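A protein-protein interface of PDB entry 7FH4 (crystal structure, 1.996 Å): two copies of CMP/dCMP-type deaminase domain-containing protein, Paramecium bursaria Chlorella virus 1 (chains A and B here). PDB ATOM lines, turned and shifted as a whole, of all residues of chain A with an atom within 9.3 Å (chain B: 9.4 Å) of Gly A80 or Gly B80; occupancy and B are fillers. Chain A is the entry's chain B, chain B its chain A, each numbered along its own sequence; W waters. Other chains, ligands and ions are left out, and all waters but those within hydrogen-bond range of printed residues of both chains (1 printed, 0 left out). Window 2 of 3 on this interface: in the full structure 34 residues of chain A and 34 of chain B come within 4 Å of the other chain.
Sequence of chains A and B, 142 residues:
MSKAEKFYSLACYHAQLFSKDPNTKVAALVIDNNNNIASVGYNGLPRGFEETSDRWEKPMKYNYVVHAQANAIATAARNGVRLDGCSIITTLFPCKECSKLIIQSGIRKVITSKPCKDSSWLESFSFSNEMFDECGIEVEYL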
ATOM      1  N   ALA A  38      -6.214  21.669 -27.488  1.00  0.00           N
ATOM      2  CA  ALA A  38      -6.065  20.731 -26.389  1.00  0.00           C
ATOM      3  C   ALA A  38      -6.411  21.339 -25.037  1.00  0.00           C
ATOM      4  O   ALA A  38      -6.900  20.612 -24.163  1.00  0.00           O
ATOM      5  CB  ALA A  38      -4.628  20.183 -26.344  1.00  0.00           C
ATOM      6  N   SER A  39      -6.152  22.638 -24.834  1.00  0.00           N
ATOM      7  CA  SER A  39      -6.490  23.285 -23.565  1.00  0.00           C
ATOM      8  C   SER A  39      -6.570  24.793 -23.762  1.00  0.00           C
ATOM      9  O   SER A  39      -5.957  25.349 -24.670  1.00  0.00           O
ATOM     10  CB  SER A  39      -5.476  22.962 -22.457  1.00  0.00           C
ATOM     11  OG  SER A  39      -6.047  23.150 -21.157  1.00  0.00           O
ATOM     12  N   ALA A  72      -4.155  27.136 -18.333  1.00  0.00           N
ATOM     13  CA  ALA A  72      -4.359  26.157 -19.397  1.00  0.00           C
ATOM     14  C   ALA A  72      -3.616  24.856 -19.104  1.00  0.00           C
ATOM     15  O   ALA A  72      -4.104  23.767 -19.426  1.00  0.00           O
ATOM     16  CB  ALA A  72      -3.906  26.737 -20.737  1.00  0.00           C
ATOM     17  N   ILE A  73      -2.436  24.953 -18.493  1.00  0.00           N
ATOM     18  CA  ILE A  73      -1.630  23.784 -18.155  1.00  0.00           C
ATOM     19  C   ILE A  73      -2.215  23.064 -16.941  1.00  0.00           C
ATOM     20  O   ILE A  73      -2.350  21.836 -16.941  1.00  0.00           O
ATOM     21  CB  ILE A  73      -0.161  24.222 -17.927  1.00  0.00           C
ATOM     22  CG1 ILE A  73       0.497  24.638 -19.251  1.00  0.00           C
ATOM     23  CG2 ILE A  73       0.668  23.128 -17.249  1.00  0.00           C
ATOM     24  CD1 ILE A  73       1.797  25.402 -19.070  1.00  0.00           C
ATOM     25  N   ALA A  74      -2.604  23.822 -15.910  1.00  0.00           N
ATOM     26  CA  ALA A  74      -3.222  23.226 -14.731  1.00  0.00           C
ATOM     27  C   ALA A  74      -4.527  22.517 -15.078  1.00  0.00           C
ATOM     28  O   ALA A  74      -4.847  21.481 -14.486  1.00  0.00           O
ATOM     29  CB  ALA A  74      -3.468  24.300 -13.667  1.00  0.00           C
ATOM     30  N   THR A  75      -5.303  23.066 -16.023  1.00  0.00           N
ATOM     31  CA  THR A  75      -6.539  22.406 -16.446  1.00  0.00           C
ATOM     32  C   THR A  75      -6.236  21.069 -17.118  1.00  0.00           C
ATOM     33  O   THR A  75      -6.944  20.072 -16.904  1.00  0.00           O
ATOM     34  CB  THR A  75      -7.320  23.324 -17.399  1.00  0.00           C
ATOM     35  OG1 THR A  75      -7.773  24.473 -16.685  1.00  0.00           O
ATOM     36  CG2 THR A  75      -8.544  22.618 -18.023  1.00  0.00           C
ATOM     37  N   ALA A  76      -5.178  21.029 -17.928  1.00  0.00           N
ATOM     38  CA  ALA A  76      -4.787  19.785 -18.581  1.00  0.00           C
ATOM     39  C   ALA A  76      -4.357  18.740 -17.561  1.00  0.00           C
ATOM     40  O   ALA A  76      -4.663  17.553 -17.720  1.00  0.00           O
ATOM     41  CB  ALA A  76      -3.669  20.044 -19.596  1.00  0.00           C
ATOM     42  N   ALA A  77      -3.645  19.158 -16.509  1.00  0.00           N
ATOM     43  CA  ALA A  77      -3.332  18.218 -15.432  1.00  0.00           C
ATOM     44  C   ALA A  77      -4.594  17.752 -14.733  1.00  0.00           C
ATOM     45  O   ALA A  77      -4.714  16.575 -14.375  1.00  0.00           O
ATOM     46  CB  ALA A  77      -2.378  18.850 -14.419  1.00  0.00           C
ATOM     47  N   ARG A  78      -5.549  18.667 -14.520  1.00  0.00           N
ATOM     48  CA  ARG A  78      -6.788  18.303 -13.844  1.00  0.00           C
ATOM     49  C   ARG A  78      -7.555  17.248 -14.623  1.00  0.00           C
ATOM     50  O   ARG A  78      -8.043  16.270 -14.045  1.00  0.00           O
ATOM     51  CB  ARG A  78      -7.667  19.536 -13.629  1.00  0.00           C
ATOM     52  CG  ARG A  78      -8.968  19.197 -12.864  1.00  0.00           C
ATOM     53  CD  ARG A  78      -9.702  20.443 -12.408  1.00  0.00           C
ATOM     54  NE  ARG A  78     -10.769  20.091 -11.480  1.00  0.00           N
ATOM     55  CZ  ARG A  78     -11.453  20.971 -10.767  1.00  0.00           C
ATOM     56  NH1 ARG A  78     -11.188  22.270 -10.877  1.00  0.00           N
ATOM     57  NH2 ARG A  78     -12.395  20.547  -9.940  1.00  0.00           N
ATOM     58  N   ASN A  79      -7.665  17.418 -15.938  1.00  0.00           N
ATOM     59  CA  ASN A  79      -8.481  16.541 -16.759  1.00  0.00           C
ATOM     60  C   ASN A  79      -7.683  15.424 -17.416  1.00  0.00           C
ATOM     61  O   ASN A  79      -8.270  14.600 -18.126  1.00  0.00           O
ATOM     62  CB  ASN A  79      -9.212  17.360 -17.825  1.00  0.00           C
ATOM     63  CG  ASN A  79     -10.147  18.403 -17.221  1.00  0.00           C
ATOM     64  OD1 ASN A  79     -10.490  18.344 -16.034  1.00  0.00           O
ATOM     65  ND2 ASN A  79     -10.568  19.362 -18.040  1.00  0.00           N
ATOM     66  N   GLY A  80      -6.366  15.367 -17.192  1.00  0.00           N
ATOM     67  CA  GLY A  80      -5.549  14.346 -17.831  1.00  0.00           C
ATOM     68  C   GLY A  80      -5.490  14.481 -19.344  1.00  0.00           C
ATOM     69  O   GLY A  80      -5.666  13.495 -20.063  1.00  0.00           O
ATOM     70  N   VAL A  81      -5.270  15.694 -19.845  1.00  0.00           N
ATOM     71  CA  VAL A  81      -5.165  15.947 -21.281  1.00  0.00           C
ATOM     72  C   VAL A  81      -3.697  16.171 -21.602  1.00  0.00           C
ATOM     73  O   VAL A  81      -3.093  17.138 -21.119  1.00  0.00           O
ATOM     74  CB  VAL A  81      -6.006  17.154 -21.711  1.00  0.00           C
ATOM     75  CG1 VAL A  81      -5.730  17.489 -23.181  1.00  0.00           C
ATOM     76  CG2 VAL A  81      -7.499  16.878 -21.465  1.00  0.00           C
ATOM     77  N   ARG A  82      -3.124  15.298 -22.422  1.00  0.00           N
ATOM     78  CA  ARG A  82      -1.690  15.375 -22.660  1.00  0.00           C
ATOM     79  C   ARG A  82      -1.333  16.554 -23.555  1.00  0.00           C
ATOM     80  O   ARG A  82      -1.921  16.741 -24.622  1.00  0.00           O
ATOM     81  CB  ARG A  82      -1.178  14.092 -23.290  1.00  0.00           C
ATOM     82  CG  ARG A  82       0.195  14.323 -23.883  1.00  0.00           C
ATOM     83  CD  ARG A  82       0.167  14.092 -25.350  1.00  0.00           C
ATOM     84  NE  ARG A  82      -0.374  12.766 -25.527  1.00  0.00           N
ATOM     85  CZ  ARG A  82       0.300  11.670 -25.218  1.00  0.00           C
ATOM     86  NH1 ARG A  82       1.540  11.743 -24.745  1.00  0.00           N
ATOM     87  NH2 ARG A  82      -0.262  10.502 -25.384  1.00  0.00           N
ATOM     88  N   LEU A  83      -0.326  17.322 -23.137  1.00  0.00           N
ATOM     89  CA  LEU A  83       0.123  18.498 -23.863  1.00  0.00           C
ATOM     90  C   LEU A  83       1.475  18.311 -24.540  1.00  0.00           C
ATOM     91  O   LEU A  83       1.908  19.212 -25.264  1.00  0.00           O
ATOM     92  CB  LEU A  83       0.197  19.706 -22.913  1.00  0.00           C
ATOM     93  CG  LEU A  83      -1.093  20.049 -22.162  1.00  0.00           C
ATOM     94  CD1 LEU A  83      -0.880  21.316 -21.354  1.00  0.00           C
ATOM     95  CD2 LEU A  83      -2.271  20.218 -23.138  1.00  0.00           C
ATOM     96  N   ASP A  84       2.143  17.181 -24.328  1.00  0.00           N
ATOM     97  CA  ASP A  84       3.492  16.959 -24.864  1.00  0.00           C
ATOM     98  C   ASP A  84       3.548  17.187 -26.374  1.00  0.00           C
ATOM     99  O   ASP A  84       2.851  16.519 -27.139  1.00  0.00           O
ATOM    100  CB  ASP A  84       3.932  15.533 -24.538  1.00  0.00           C
ATOM    101  CG  ASP A  84       5.436  15.333 -24.674  1.00  0.00           C
ATOM    102  OD1 ASP A  84       6.197  16.320 -24.658  1.00  0.00           O
ATOM    103  OD2 ASP A  84       5.862  14.175 -24.780  1.00  0.00           O
ATOM    104  N   SER A 105       5.980  21.152 -19.242  1.00  0.00           N
ATOM    105  CA  SER A 105       4.817  20.430 -19.741  1.00  0.00           C
ATOM    106  C   SER A 105       4.996  19.942 -21.178  1.00  0.00           C
ATOM    107  O   SER A 105       4.028  19.464 -21.776  1.00  0.00           O
ATOM    108  CB  SER A 105       3.560  21.303 -19.629  1.00  0.00           C
ATOM    109  OG  SER A 105       3.608  22.363 -20.562  1.00  0.00           O
ATOM    110  N   ALA B  38       0.019   9.167  -8.639  1.00  0.00           N
ATOM    111  CA  ALA B  38      -0.350   9.711  -9.933  1.00  0.00           C
ATOM    112  C   ALA B  38       0.729  10.591 -10.540  1.00  0.00           C
ATOM    113  O   ALA B  38       0.845  10.633 -11.766  1.00  0.00           O
ATOM    114  CB  ALA B  38      -1.644  10.525  -9.815  1.00  0.00           C
ATOM    115  N   SER B  39       1.508  11.306  -9.724  1.00  0.00           N
ATOM    116  CA  SER B  39       2.553  12.177 -10.253  1.00  0.00           C
ATOM    117  C   SER B  39       3.561  12.495  -9.158  1.00  0.00           C
ATOM    118  O   SER B  39       3.260  12.423  -7.963  1.00  0.00           O
ATOM    119  CB  SER B  39       1.974  13.473 -10.824  1.00  0.00           C
ATOM    120  OG  SER B  39       2.859  14.021 -11.775  1.00  0.00           O
ATOM    121  N   ALA B  72       5.282  18.417 -10.402  1.00  0.00           N
ATOM    122  CA  ALA B  72       4.363  17.283 -10.399  1.00  0.00           C
ATOM    123  C   ALA B  72       3.126  17.577 -11.242  1.00  0.00           C
ATOM    124  O   ALA B  72       2.598  16.685 -11.919  1.00  0.00           O
ATOM    125  CB  ALA B  72       3.966  16.905  -8.972  1.00  0.00           C
ATOM    126  N   ILE B  73       2.671  18.827 -11.242  1.00  0.00           N
ATOM    127  CA  ILE B  73       1.471  19.176 -11.991  1.00  0.00           C
ATOM    128  C   ILE B  73       1.793  19.341 -13.472  1.00  0.00           C
ATOM    129  O   ILE B  73       1.048  18.862 -14.338  1.00  0.00           O
ATOM    130  CB  ILE B  73       0.845  20.444 -11.383  1.00  0.00           C
ATOM    131  CG1 ILE B  73       0.293  20.128  -9.974  1.00  0.00           C
ATOM    132  CG2 ILE B  73      -0.211  21.018 -12.312  1.00  0.00           C
ATOM    133  CD1 ILE B  73      -0.081  21.354  -9.154  1.00  0.00           C
ATOM    134  N   ALA B  74       2.924  19.981 -13.783  1.00  0.00           N
ATOM    135  CA  ALA B  74       3.332  20.131 -15.177  1.00  0.00           C
ATOM    136  C   ALA B  74       3.585  18.778 -15.821  1.00  0.00           C
ATOM    137  O   ALA B  74       3.303  18.589 -17.011  1.00  0.00           O
ATOM    138  CB  ALA B  74       4.575  21.012 -15.276  1.00  0.00           C
ATOM    139  N   THR B  75       4.131  17.827 -15.057  1.00  0.00           N
ATOM    140  CA  THR B  75       4.390  16.501 -15.607  1.00  0.00           C
ATOM    141  C   THR B  75       3.084  15.799 -15.946  1.00  0.00           C
ATOM    142  O   THR B  75       2.980  15.125 -16.980  1.00  0.00           O
ATOM    143  CB  THR B  75       5.205  15.668 -14.618  1.00  0.00           C
ATOM    144  OG1 THR B  75       6.511  16.228 -14.489  1.00  0.00           O
ATOM    145  CG2 THR B  75       5.324  14.216 -15.085  1.00  0.00           C
ATOM    146  N   ALA B  76       2.070  15.965 -15.090  1.00  0.00           N
ATOM    147  CA  ALA B  76       0.761  15.388 -15.358  1.00  0.00           C
ATOM    148  C   ALA B  76       0.128  16.029 -16.589  1.00  0.00           C
ATOM    149  O   ALA B  76      -0.510  15.339 -17.396  1.00  0.00           O
ATOM    150  CB  ALA B  76      -0.146  15.548 -14.129  1.00  0.00           C
ATOM    151  N   ALA B  77       0.297  17.347 -16.754  1.00  0.00           N
ATOM    152  CA  ALA B  77      -0.160  17.990 -17.984  1.00  0.00           C
ATOM    153  C   ALA B  77       0.587  17.448 -19.193  1.00  0.00           C
ATOM    154  O   ALA B  77      -0.019  17.185 -20.240  1.00  0.00           O
ATOM    155  CB  ALA B  77       0.014  19.507 -17.886  1.00  0.00           C
ATOM    156  N   ARG B  78       1.908  17.276 -19.066  1.00  0.00           N
ATOM    157  CA  ARG B  78       2.701  16.775 -20.186  1.00  0.00           C
ATOM    158  C   ARG B  78       2.267  15.379 -20.602  1.00  0.00           C
ATOM    159  O   ARG B  78       2.192  15.075 -21.799  1.00  0.00           O
ATOM    160  CB  ARG B  78       4.185  16.760 -19.827  1.00  0.00           C
ATOM    161  CG  ARG B  78       5.078  16.234 -20.982  1.00  0.00           C
ATOM    162  CD  ARG B  78       6.561  16.364 -20.632  1.00  0.00           C
ATOM    163  NE  ARG B  78       7.370  16.227 -21.824  1.00  0.00           N
ATOM    164  CZ  ARG B  78       8.573  16.761 -21.995  1.00  0.00           C
ATOM    165  NH1 ARG B  78       9.143  17.479 -21.035  1.00  0.00           N
ATOM    166  NH2 ARG B  78       9.202  16.576 -23.145  1.00  0.00           N
ATOM    167  N   ASN B  79       2.007  14.509 -19.633  1.00  0.00           N
ATOM    168  CA  ASN B  79       1.741  13.113 -19.923  1.00  0.00           C
ATOM    169  C   ASN B  79       0.257  12.792 -19.986  1.00  0.00           C
ATOM    170  O   ASN B  79      -0.095  11.654 -20.286  1.00  0.00           O
ATOM    171  CB  ASN B  79       2.424  12.222 -18.883  1.00  0.00           C
ATOM    172  CG  ASN B  79       3.934  12.319 -18.949  1.00  0.00           C
ATOM    173  OD1 ASN B  79       4.487  12.815 -19.937  1.00  0.00           O
ATOM    174  ND2 ASN B  79       4.612  11.836 -17.903  1.00  0.00           N
ATOM    175  N   GLY B  80      -0.617  13.762 -19.737  1.00  0.00           N
ATOM    176  CA  GLY B  80      -2.046  13.461 -19.701  1.00  0.00           C
ATOM    177  C   GLY B  80      -2.471  12.544 -18.573  1.00  0.00           C
ATOM    178  O   GLY B  80      -3.272  11.630 -18.795  1.00  0.00           O
ATOM    179  N   VAL B  81      -1.944  12.752 -17.368  1.00  0.00           N
ATOM    180  CA  VAL B  81      -2.363  12.003 -16.187  1.00  0.00           C
ATOM    181  C   VAL B  81      -3.334  12.871 -15.402  1.00  0.00           C
ATOM    182  O   VAL B  81      -2.984  13.982 -14.981  1.00  0.00           O
ATOM    183  CB  VAL B  81      -1.163  11.600 -15.314  1.00  0.00           C
ATOM    184  CG1 VAL B  81      -1.650  10.830 -14.093  1.00  0.00           C
ATOM    185  CG2 VAL B  81      -0.198  10.776 -16.096  1.00  0.00           C
ATOM    186  N   ARG B  82      -4.540  12.357 -15.180  1.00  0.00           N
ATOM    187  CA  ARG B  82      -5.629  13.134 -14.591  1.00  0.00           C
ATOM    188  C   ARG B  82      -5.420  13.273 -13.081  1.00  0.00           C
ATOM    189  O   ARG B  82      -5.353  12.273 -12.365  1.00  0.00           O
ATOM    190  CB  ARG B  82      -6.960  12.447 -14.925  1.00  0.00           C
ATOM    191  CG  ARG B  82      -8.092  12.658 -13.950  1.00  0.00           C
ATOM    192  CD  ARG B  82      -9.352  11.904 -14.401  1.00  0.00           C
ATOM    193  NE  ARG B  82     -10.140  12.683 -15.353  1.00  0.00           N
ATOM    194  CZ  ARG B  82     -10.152  12.479 -16.671  1.00  0.00           C
ATOM    195  NH1 ARG B  82      -9.422  11.505 -17.203  1.00  0.00           N
ATOM    196  NH2 ARG B  82     -10.900  13.249 -17.458  1.00  0.00           N
ATOM    197  N   LEU B  83      -5.311  14.509 -12.594  1.00  0.00           N
ATOM    198  CA  LEU B  83      -5.063  14.748 -11.173  1.00  0.00           C
ATOM    199  C   LEU B  83      -6.309  15.124 -10.369  1.00  0.00           C
ATOM    200  O   LEU B  83      -6.224  15.256  -9.136  1.00  0.00           O
ATOM    201  CB  LEU B  83      -4.023  15.849 -11.004  1.00  0.00           C
ATOM    202  CG  LEU B  83      -2.650  15.520 -11.594  1.00  0.00           C
ATOM    203  CD1 LEU B  83      -1.638  16.543 -11.095  1.00  0.00           C
ATOM    204  CD2 LEU B  83      -2.234  14.088 -11.238  1.00  0.00           C
ATOM    205  N   ASP B  84      -7.446  15.321 -11.026  1.00  0.00           N
ATOM    206  CA  ASP B  84      -8.632  15.836 -10.345  1.00  0.00           C
ATOM    207  C   ASP B  84      -8.987  14.967  -9.142  1.00  0.00           C
ATOM    208  O   ASP B  84      -9.093  13.746  -9.261  1.00  0.00           O
ATOM    209  CB  ASP B  84      -9.803  15.881 -11.324  1.00  0.00           C
ATOM    210  CG  ASP B  84     -11.032  16.528 -10.719  1.00  0.00           C
ATOM    211  OD1 ASP B  84     -10.909  17.640 -10.174  1.00  0.00           O
ATOM    212  OD2 ASP B  84     -12.104  15.904 -10.754  1.00  0.00           O
ATOM    213  N   SER B 105      -5.704  22.660 -10.504  1.00  0.00           N
ATOM    214  CA  SER B 105      -5.547  21.311 -11.027  1.00  0.00           C
ATOM    215  C   SER B 105      -6.485  20.317 -10.366  1.00  0.00           C
ATOM    216  O   SER B 105      -6.400  19.121 -10.657  1.00  0.00           O
ATOM    217  CB  SER B 105      -4.093  20.838 -10.872  1.00  0.00           C
ATOM    218  OG  SER B 105      -3.774  20.612  -9.516  1.00  0.00           O
HETATM  219  O   HOH W   1       8.439  14.020 -24.647  1.00  0.00           O
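O of Val A81 lies close to O of Ala B77 (3.2 Å).
O of Gly B80 sits close to O of Gly A80, at 3.3 Å.
The backbone carbonyl oxygen of Ala A77 lies within hydrogen-bond range of the backbone NH of Leu B83 (2.8 Å).
The backbone carbonyl oxygen (O) of Ala A77 sits close to the backbone carbonyl oxygen (O) of Val B81, at 3.2 Å.
O of Asn A79 sits at hydrogen-bond distance from NH2 of Arg B82 (3.0 Å).
The backbone carbonyl oxygen (O) of Ala B77 lies within hydrogen-bond range of the backbone NH (N) of Leu A83 (2.9 Å).
The side-chain carboxylate of Asp A84 lies within salt-bridge range of the guanidinium group of Arg B78, at 3.1 Å.
The side-chain carboxylate of Asp B84 is in salt-bridge range of the guanidinium group of Arg A78 (2.8 Å).
N of Val A81 sits at hydrogen-bond distance from O of Ala A76, 2.9 Å away.
The backbone NH of Val B81 lies within hydrogen-bond range of the backbone carbonyl oxygen of Ala B76 (3.0 Å).
Among the printed residues, pairs that only touch across the chains: Ile A73 with Ala B77, Ala A74 with Ser B105, Ala A77 with Ile B73, Ala A77 with Ala B76, Ala A77 with Ala B77, Ala A77 with Arg B82, Arg A78 with Arg B82, Arg A78 with Leu B83, Arg A78 with Ser B105, Gly A80 with Val B81, Gly A80 with Arg B82, Val A81 with Gly B80, Arg A82 with Ala B77, Arg A82 with Arg B78, Arg A82 with Asn B79, Arg A82 with Gly B80, Leu A83 with Arg B78, Ser A105 with Ala B74 and Ser A105 with Arg B78.
Ala A38 touches none of the printed residues of chain B.
Of the printed residues of chain B, Asn A79 touches Arg B82 (3.0 Å).
Gly A80 touches three residues of chain B.
Of the printed residues of chain B, Leu A83 touches Ala B77 (2.9 Å) and Arg B78 (3.6 Å).
Ala B72 touches none of the printed residues of chain A.
Of the printed residues of chain A, Ile B73 touches Ala A77.
Of the printed residues of chain A, Asn B79 touches Arg A82.
Of the printed residues of chain A, Arg B82 touches Ala A77, Arg A78, Asn A79 and Gly A80.
The nearest residue of chain B that does not touch Gly A80 is Leu B83 (4.8 Å).
The nearest residue of chain A that does not touch Gly B80 is Leu A83 (4.9 Å).
Of the 16 printed residues of chain A, 11 touch a printed residue of chain B.
Hydrophobic or aromatic side chains of chain A within 4 Å of the printed part of chain B: Ile A73, Ala A77 and Leu A83.
Among the printed residues, 27 pairs touch across the chains.
Among the printed residues, Asp or Glu carboxylates within 4 Å of a Lys or Arg side-chain nitrogen of the other chain: Arg A78 with Asp B84 and Asp A84 with Arg B78.
Ala A77 touches its own counterpart, Ala B77.
Ala A77 touches Leu B83, and with the chains exchanged Leu A83 touches Ala B77.
Arg A78 touches Leu B83, and with the chains exchanged Leu A83 touches Arg B78.
Arg A78 touches Asp B84, and with the chains exchanged Asp A84 touches Arg B78.
16 positions are printed for both chains.
Water W1 lies within hydrogen-bond range of OD2 of Asp A84 (2.6 Å) and NH2 of Arg B78 (3.1 Å).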
